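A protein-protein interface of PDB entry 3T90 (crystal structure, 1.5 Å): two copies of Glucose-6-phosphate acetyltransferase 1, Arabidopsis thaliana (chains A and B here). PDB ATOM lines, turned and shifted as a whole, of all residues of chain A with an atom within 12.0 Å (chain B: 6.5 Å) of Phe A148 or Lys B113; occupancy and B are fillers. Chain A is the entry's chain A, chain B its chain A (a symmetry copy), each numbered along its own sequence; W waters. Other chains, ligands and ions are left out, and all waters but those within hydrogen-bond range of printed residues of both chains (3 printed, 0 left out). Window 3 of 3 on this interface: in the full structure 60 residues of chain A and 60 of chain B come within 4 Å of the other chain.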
ATOM      1  N   MET A 144     -10.124   2.954  11.627  1.00  0.00           N
ATOM      2  CA  MET A 144      -9.660   3.169  13.008  1.00  0.00           C
ATOM      3  C   MET A 144      -9.905   1.883  13.804  1.00  0.00           C
ATOM      4  O   MET A 144     -10.883   1.178  13.579  1.00  0.00           O
ATOM      5  CB  MET A 144     -10.447   4.306  13.693  1.00  0.00           C
ATOM      6  CG  MET A 144     -10.440   5.657  13.050  1.00  0.00           C
ATOM      7  SD  MET A 144      -8.810   6.355  12.772  1.00  0.00           S
ATOM      8  CE  MET A 144      -8.216   6.583  14.425  1.00  0.00           C
ATOM      9  N   SER A 145      -9.003   1.584  14.738  1.00  0.00           N
ATOM     10  CA  SER A 145      -9.148   0.382  15.527  1.00  0.00           C
ATOM     11  C   SER A 145      -8.764   0.615  16.989  1.00  0.00           C
ATOM     12  O   SER A 145      -7.933   1.480  17.296  1.00  0.00           O
ATOM     13  CB  SER A 145      -8.207  -0.705  14.965  1.00  0.00           C
ATOM     14  OG  SER A 145      -6.816  -0.254  14.975  1.00  0.00           O
ATOM     15  N   LYS A 146      -9.369  -0.166  17.843  1.00  0.00           N
ATOM     16  CA  LYS A 146      -8.990  -0.204  19.294  1.00  0.00           C
ATOM     17  C   LYS A 146      -8.988  -1.664  19.681  1.00  0.00           C
ATOM     18  O   LYS A 146      -9.985  -2.338  19.566  1.00  0.00           O
ATOM     19  CB  LYS A 146      -9.980   0.536  20.169  1.00  0.00           C
ATOM     20  CG  LYS A 146      -9.555   0.406  21.677  1.00  0.00           C
ATOM     21  CD  LYS A 146     -10.561   1.185  22.571  1.00  0.00           C
ATOM     22  CE  LYS A 146     -10.061   1.377  24.020  1.00  0.00           C
ATOM     23  NZ  LYS A 146     -10.679   2.754  24.267  1.00  0.00           N
ATOM     24  N   TYR A 147      -7.834  -2.149  20.146  1.00  0.00           N
ATOM     25  CA  TYR A 147      -7.707  -3.479  20.680  1.00  0.00           C
ATOM     26  C   TYR A 147      -7.825  -3.425  22.201  1.00  0.00           C
ATOM     27  O   TYR A 147      -7.236  -2.554  22.852  1.00  0.00           O
ATOM     28  CB  TYR A 147      -6.313  -4.067  20.287  1.00  0.00           C
ATOM     29  CG  TYR A 147      -6.256  -4.530  18.862  1.00  0.00           C
ATOM     30  CD1 TYR A 147      -6.191  -5.880  18.574  1.00  0.00           C
ATOM     31  CD2 TYR A 147      -6.359  -3.616  17.794  1.00  0.00           C
ATOM     32  CE1 TYR A 147      -6.202  -6.381  17.249  1.00  0.00           C
ATOM     33  CE2 TYR A 147      -6.324  -4.121  16.394  1.00  0.00           C
ATOM     34  CZ  TYR A 147      -6.305  -5.492  16.194  1.00  0.00           C
ATOM     35  OH  TYR A 147      -6.276  -5.928  14.913  1.00  0.00           O
ATOM     36  N   PHE A 148      -8.467  -4.437  22.740  1.00  0.00           N
ATOM     37  CA  PHE A 148      -8.669  -4.614  24.181  1.00  0.00           C
ATOM     38  C   PHE A 148      -7.560  -5.564  24.686  1.00  0.00           C
ATOM     39  O   PHE A 148      -7.837  -6.429  25.502  1.00  0.00           O
ATOM     40  CB  PHE A 148     -10.060  -5.105  24.511  1.00  0.00           C
ATOM     41  CG  PHE A 148     -11.151  -4.202  24.010  1.00  0.00           C
ATOM     42  CD1 PHE A 148     -11.335  -2.919  24.529  1.00  0.00           C
ATOM     43  CD2 PHE A 148     -12.037  -4.678  23.034  1.00  0.00           C
ATOM     44  CE1 PHE A 148     -12.374  -2.145  23.973  1.00  0.00           C
ATOM     45  CE2 PHE A 148     -13.039  -3.959  22.554  1.00  0.00           C
ATOM     46  CZ  PHE A 148     -13.207  -2.678  22.962  1.00  0.00           C
ATOM     47  N   ASP A 149      -6.325  -5.332  24.274  1.00  0.00           N
ATOM     48  CA  ASP A 149      -5.227  -6.224  24.634  1.00  0.00           C
ATOM     49  C   ASP A 149      -4.930  -5.980  26.089  1.00  0.00           C
ATOM     50  O   ASP A 149      -4.326  -6.854  26.777  1.00  0.00           O
ATOM     51  CB  ASP A 149      -3.967  -5.962  23.806  1.00  0.00           C
ATOM     52  CG  ASP A 149      -4.098  -6.310  22.350  1.00  0.00           C
ATOM     53  OD1 ASP A 149      -3.546  -5.517  21.530  1.00  0.00           O
ATOM     54  OD2 ASP A 149      -4.641  -7.406  22.043  1.00  0.00           O
ATOM     55  N   ARG B  78      -7.789 -15.445  16.399  1.00  0.00           N
ATOM     56  CA  ARG B  78      -7.878 -14.890  17.729  1.00  0.00           C
ATOM     57  C   ARG B  78      -8.634 -15.828  18.699  1.00  0.00           C
ATOM     58  O   ARG B  78      -9.412 -15.434  19.503  1.00  0.00           O
ATOM     59  CB  ARG B  78      -8.406 -13.408  17.758  1.00  0.00           C
ATOM     60  CG  ARG B  78      -7.331 -12.392  17.303  1.00  0.00           C
ATOM     61  CD  ARG B  78      -6.475 -12.099  18.584  1.00  0.00           C
ATOM     62  NE  ARG B  78      -5.688 -10.853  18.502  1.00  0.00           N
ATOM     63  CZ  ARG B  78      -5.499 -10.068  19.540  1.00  0.00           C
ATOM     64  NH1 ARG B  78      -6.028 -10.423  20.782  1.00  0.00           N
ATOM     65  NH2 ARG B  78      -4.747  -8.953  19.375  1.00  0.00           N
ATOM     66  N   LEU B 108     -20.677   1.982  22.661  1.00  0.00           N
ATOM     67  CA  LEU B 108     -20.484   0.795  21.867  1.00  0.00           C
ATOM     68  C   LEU B 108     -19.186   0.071  22.179  1.00  0.00           C
ATOM     69  O   LEU B 108     -19.213  -1.170  22.135  1.00  0.00           O
ATOM     70  CB  LEU B 108     -20.497   1.244  20.406  1.00  0.00           C
ATOM     71  CG  LEU B 108     -21.771   1.982  19.944  1.00  0.00           C
ATOM     72  CD1 LEU B 108     -21.602   2.636  18.562  1.00  0.00           C
ATOM     73  CD2 LEU B 108     -22.939   0.982  19.850  1.00  0.00           C
ATOM     74  N   MET B 109     -18.122   0.799  22.497  1.00  0.00           N
ATOM     75  CA  MET B 109     -16.873   0.101  22.893  1.00  0.00           C
ATOM     76  C   MET B 109     -17.092  -0.628  24.203  1.00  0.00           C
ATOM     77  O   MET B 109     -16.681  -1.795  24.349  1.00  0.00           O
ATOM     78  CB  MET B 109     -15.783   1.121  23.075  1.00  0.00           C
ATOM     79  CG  MET B 109     -15.303   1.690  21.774  1.00  0.00           C
ATOM     80  SD  MET B 109     -14.086   3.011  22.201  1.00  0.00           S
ATOM     81  CE  MET B 109     -13.428   3.038  20.571  1.00  0.00           C
ATOM     82  N   ASP B 110     -17.815   0.000  25.111  1.00  0.00           N
ATOM     83  CA  ASP B 110     -18.070  -0.664  26.411  1.00  0.00           C
ATOM     84  C   ASP B 110     -18.855  -1.972  26.211  1.00  0.00           C
ATOM     85  O   ASP B 110     -18.582  -3.036  26.761  1.00  0.00           O
ATOM     86  CB  ASP B 110     -18.916   0.267  27.335  1.00  0.00           C
ATOM     87  CG  ASP B 110     -18.148   1.456  27.892  1.00  0.00           C
ATOM     88  OD1 ASP B 110     -16.906   1.485  27.873  1.00  0.00           O
ATOM     89  OD2 ASP B 110     -18.883   2.393  28.320  1.00  0.00           O
ATOM     90  N   HIS B 111     -19.855  -1.958  25.322  1.00  0.00           N
ATOM     91  CA  HIS B 111     -20.600  -3.139  25.019  1.00  0.00           C
ATOM     92  C   HIS B 111     -19.673  -4.242  24.424  1.00  0.00           C
ATOM     93  O   HIS B 111     -19.714  -5.418  24.848  1.00  0.00           O
ATOM     94  CB  HIS B 111     -21.693  -2.770  23.965  1.00  0.00           C
ATOM     95  CG  HIS B 111     -22.500  -3.956  23.614  1.00  0.00           C
ATOM     96  ND1 HIS B 111     -23.361  -4.583  24.513  1.00  0.00           N
ATOM     97  CD2 HIS B 111     -22.482  -4.728  22.495  1.00  0.00           C
ATOM     98  CE1 HIS B 111     -23.895  -5.637  23.912  1.00  0.00           C
ATOM     99  NE2 HIS B 111     -23.362  -5.762  22.709  1.00  0.00           N
ATOM    100  N   CYS B 112     -18.845  -3.870  23.473  1.00  0.00           N
ATOM    101  CA  CYS B 112     -18.012  -4.883  22.863  1.00  0.00           C
ATOM    102  C   CYS B 112     -16.988  -5.436  23.871  1.00  0.00           C
ATOM    103  O   CYS B 112     -16.737  -6.645  23.824  1.00  0.00           O
ATOM    104  CB  CYS B 112     -17.236  -4.295  21.740  1.00  0.00           C
ATOM    105  SG  CYS B 112     -18.304  -3.942  20.294  1.00  0.00           S
ATOM    106  N   LYS B 113     -16.430  -4.608  24.760  1.00  0.00           N
ATOM    107  CA  LYS B 113     -15.453  -5.098  25.744  1.00  0.00           C
ATOM    108  C   LYS B 113     -16.182  -6.079  26.640  1.00  0.00           C
ATOM    109  O   LYS B 113     -15.668  -7.209  26.927  1.00  0.00           O
ATOM    110  CB  LYS B 113     -14.893  -3.945  26.521  1.00  0.00           C
ATOM    111  CG  LYS B 113     -13.823  -4.499  27.451  1.00  0.00           C
ATOM    112  CD  LYS B 113     -13.455  -3.501  28.505  1.00  0.00           C
ATOM    113  CE  LYS B 113     -12.777  -2.307  28.051  1.00  0.00           C
ATOM    114  NZ  LYS B 113     -12.242  -1.761  29.368  1.00  0.00           N
ATOM    115  N   SER B 114     -17.403  -5.731  27.059  1.00  0.00           N
ATOM    116  CA  SER B 114     -18.198  -6.599  27.911  1.00  0.00           C
ATOM    117  C   SER B 114     -18.599  -7.938  27.258  1.00  0.00           C
ATOM    118  O   SER B 114     -18.724  -8.951  27.938  1.00  0.00           O
ATOM    119  CB  SER B 114     -19.448  -5.858  28.404  1.00  0.00           C
ATOM    120  OG  SER B 114     -20.455  -5.805  27.423  1.00  0.00           O
ATOM    121  N   MET B 115     -18.761  -7.949  25.939  1.00  0.00           N
ATOM    122  CA  MET B 115     -19.051  -9.170  25.208  1.00  0.00           C
ATOM    123  C   MET B 115     -17.828 -10.022  24.903  1.00  0.00           C
ATOM    124  O   MET B 115     -17.950 -11.046  24.219  1.00  0.00           O
ATOM    125  CB  MET B 115     -19.780  -8.807  23.854  1.00  0.00           C
ATOM    126  CG  MET B 115     -21.097  -8.138  24.118  1.00  0.00           C
ATOM    127  SD  MET B 115     -22.327  -9.275  24.789  1.00  0.00           S
ATOM    128  CE  MET B 115     -22.546 -10.336  23.368  1.00  0.00           C
ATOM    129  N   GLY B 116     -16.671  -9.554  25.335  1.00  0.00           N
ATOM    130  CA  GLY B 116     -15.444 -10.303  25.123  1.00  0.00           C
ATOM    131  C   GLY B 116     -14.843 -10.157  23.747  1.00  0.00           C
ATOM    132  O   GLY B 116     -14.060 -10.993  23.329  1.00  0.00           O
ATOM    133  N   CYS B 117     -15.101  -9.040  23.093  1.00  0.00           N
ATOM    134  CA  CYS B 117     -14.469  -8.835  21.762  1.00  0.00           C
ATOM    135  C   CYS B 117     -12.965  -8.514  21.984  1.00  0.00           C
ATOM    136  O   CYS B 117     -12.573  -7.906  23.051  1.00  0.00           O
ATOM    137  CB  CYS B 117     -15.030  -7.584  21.068  1.00  0.00           C
ATOM    138  SG  CYS B 117     -16.731  -7.800  20.504  1.00  0.00           S
ATOM    139  N   TYR B 118     -12.108  -8.867  21.023  1.00  0.00           N
ATOM    140  CA  TYR B 118     -10.664  -8.515  21.196  1.00  0.00           C
ATOM    141  C   TYR B 118     -10.337  -7.133  20.572  1.00  0.00           C
ATOM    142  O   TYR B 118      -9.283  -6.564  20.871  1.00  0.00           O
ATOM    143  CB  TYR B 118      -9.778  -9.626  20.592  1.00  0.00           C
ATOM    144  CG  TYR B 118      -9.854  -9.763  19.071  1.00  0.00           C
ATOM    145  CD1 TYR B 118      -9.000  -9.077  18.250  1.00  0.00           C
ATOM    146  CD2 TYR B 118     -10.817 -10.550  18.514  1.00  0.00           C
ATOM    147  CE1 TYR B 118      -9.095  -9.206  16.826  1.00  0.00           C
ATOM    148  CE2 TYR B 118     -10.932 -10.680  17.156  1.00  0.00           C
ATOM    149  CZ  TYR B 118     -10.051 -10.045  16.314  1.00  0.00           C
ATOM    150  OH  TYR B 118     -10.203 -10.152  14.921  1.00  0.00           O
ATOM    151  N   LYS B 119     -11.258  -6.610  19.713  1.00  0.00           N
ATOM    152  CA  LYS B 119     -11.067  -5.330  19.110  1.00  0.00           C
ATOM    153  C   LYS B 119     -12.403  -4.775  18.668  1.00  0.00           C
ATOM    154  O   LYS B 119     -13.400  -5.502  18.534  1.00  0.00           O
ATOM    155  CB  LYS B 119     -10.084  -5.408  17.890  1.00  0.00           C
ATOM    156  CG  LYS B 119     -10.768  -5.998  16.606  1.00  0.00           C
ATOM    157  CD  LYS B 119      -9.776  -5.957  15.427  1.00  0.00           C
ATOM    158  CE  LYS B 119     -10.438  -6.563  14.173  1.00  0.00           C
ATOM    159  NZ  LYS B 119      -9.494  -6.494  12.993  1.00  0.00           N
ATOM    160  N   VAL B 120     -12.355  -3.465  18.378  1.00  0.00           N
ATOM    161  CA  VAL B 120     -13.440  -2.771  17.661  1.00  0.00           C
ATOM    162  C   VAL B 120     -12.822  -1.964  16.555  1.00  0.00           C
ATOM    163  O   VAL B 120     -11.752  -1.405  16.734  1.00  0.00           O
ATOM    164  CB  VAL B 120     -14.276  -1.916  18.577  1.00  0.00           C
ATOM    165  CG1 VAL B 120     -13.506  -0.928  19.391  1.00  0.00           C
ATOM    166  CG2 VAL B 120     -15.419  -1.344  17.901  1.00  0.00           C
HETATM  167  O   HOH W   1      -7.299  -7.525  22.099  1.00  0.00           O
HETATM  168  O   HOH W   2     -12.907   1.251  25.284  1.00  0.00           O
HETATM  169  O   HOH W   3      -7.415  -4.328  12.939  1.00  0.00           O
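The backbone carbonyl oxygen (O) of Cys B112 lies within hydrogen-bond range of the backbone NH (N) of Cys B117 (3.0 Å).
Met A144 touches none of the printed residues of chain B.
Of the printed residues of chain B, Ser A145 touches Val B120 (3.4 Å).
Printed residues of chain B within 4 Å of Tyr A147: Arg B78 (3.5 Å), Tyr B118 (3.5 Å) and Lys B119 (3.5 Å).
Of the printed residues of chain B, Phe A148 touches Met B109 (3.8 Å), Lys B113 (3.9 Å), Cys B117 (3.3 Å), Tyr B118 (2.9 Å), Lys B119 (3.9 Å) and Val B120 (3.99 Å).
His B111 touches none of the printed residues of chain A.
Lys B113 touches just one residue of chain A: Phe A148.
No residue of chain A comes within 4 Å of Gly B116.
Cys B117 touches one residue of chain A.
Of the printed residues of chain A, Tyr B118 touches Tyr A147 (3.5 Å) and Phe A148 (2.9 Å).
The nearest residue of chain A that does not touch Lys B113 is Lys A146 (6.1 Å).
The nearest printed residue of chain B that does not touch Lys A146 is Tyr B118 (4.5 Å).
Among the printed residues, pairs that only touch across the chains: Lys A146 with Lys B119, Phe A148 with Cys B117, Ser A145 with Val B120, Tyr A147 with Tyr B118, Tyr A147 with Arg B78, Tyr A147 with Lys B119, Phe A148 with Met B109, Phe A148 with Lys B113, Phe A148 with Lys B119, Lys A146 with Met B109 and Phe A148 with Val B120.
Water W1 lies within hydrogen-bond range of the backbone carbonyl oxygen of Tyr B118 (2.5 Å), the side-chain carboxylate of Asp A149 (2.7 Å), the backbone NH of Phe A148 (3.4 Å) and the guanidinium group of Arg B78 (3.4 Å).
Water W3 lies within hydrogen-bond range of OH of Tyr A147 (2.8 Å) and NZ of Lys B119 (3.0 Å).
Water W2 bridges the side-chain amino group (NZ) of Lys A146 (2.9 Å) and the side-chain sulfur (SD) of Met B109 (3.7 Å).
Of the 14 printed residues of chain B, 7 touch a printed residue of chain A.
Hydrophobic or aromatic side chains of chain B that line the printed part of chain A: Met B109 and Val B120.
Among the printed residues, 14 pairs touch across the chains.
Among the printed residues, Asp or Glu carboxylates within 4 Å of a Lys or Arg side-chain nitrogen of the other chain: Asp A149 with Arg B78 (3.1 Å).
No position is printed for both chains.
Of the 14 pairs that touch across the chains among the printed residues, none has its exchanged pair printed and touching as well.
The backbone carbonyl oxygen (O) of Lys A146 sits at hydrogen-bond distance from the backbone NH (N) of Val B120, at 2.9 Å.
The backbone carbonyl oxygen (O) of Tyr B118 sits at hydrogen-bond distance from the backbone NH (N) of Phe A148, 2.9 Å away.
The side-chain carboxylate (OD2) of Asp A149 is in salt-bridge range of the guanidinium group (NH2) of Arg B78 (3.1 Å).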
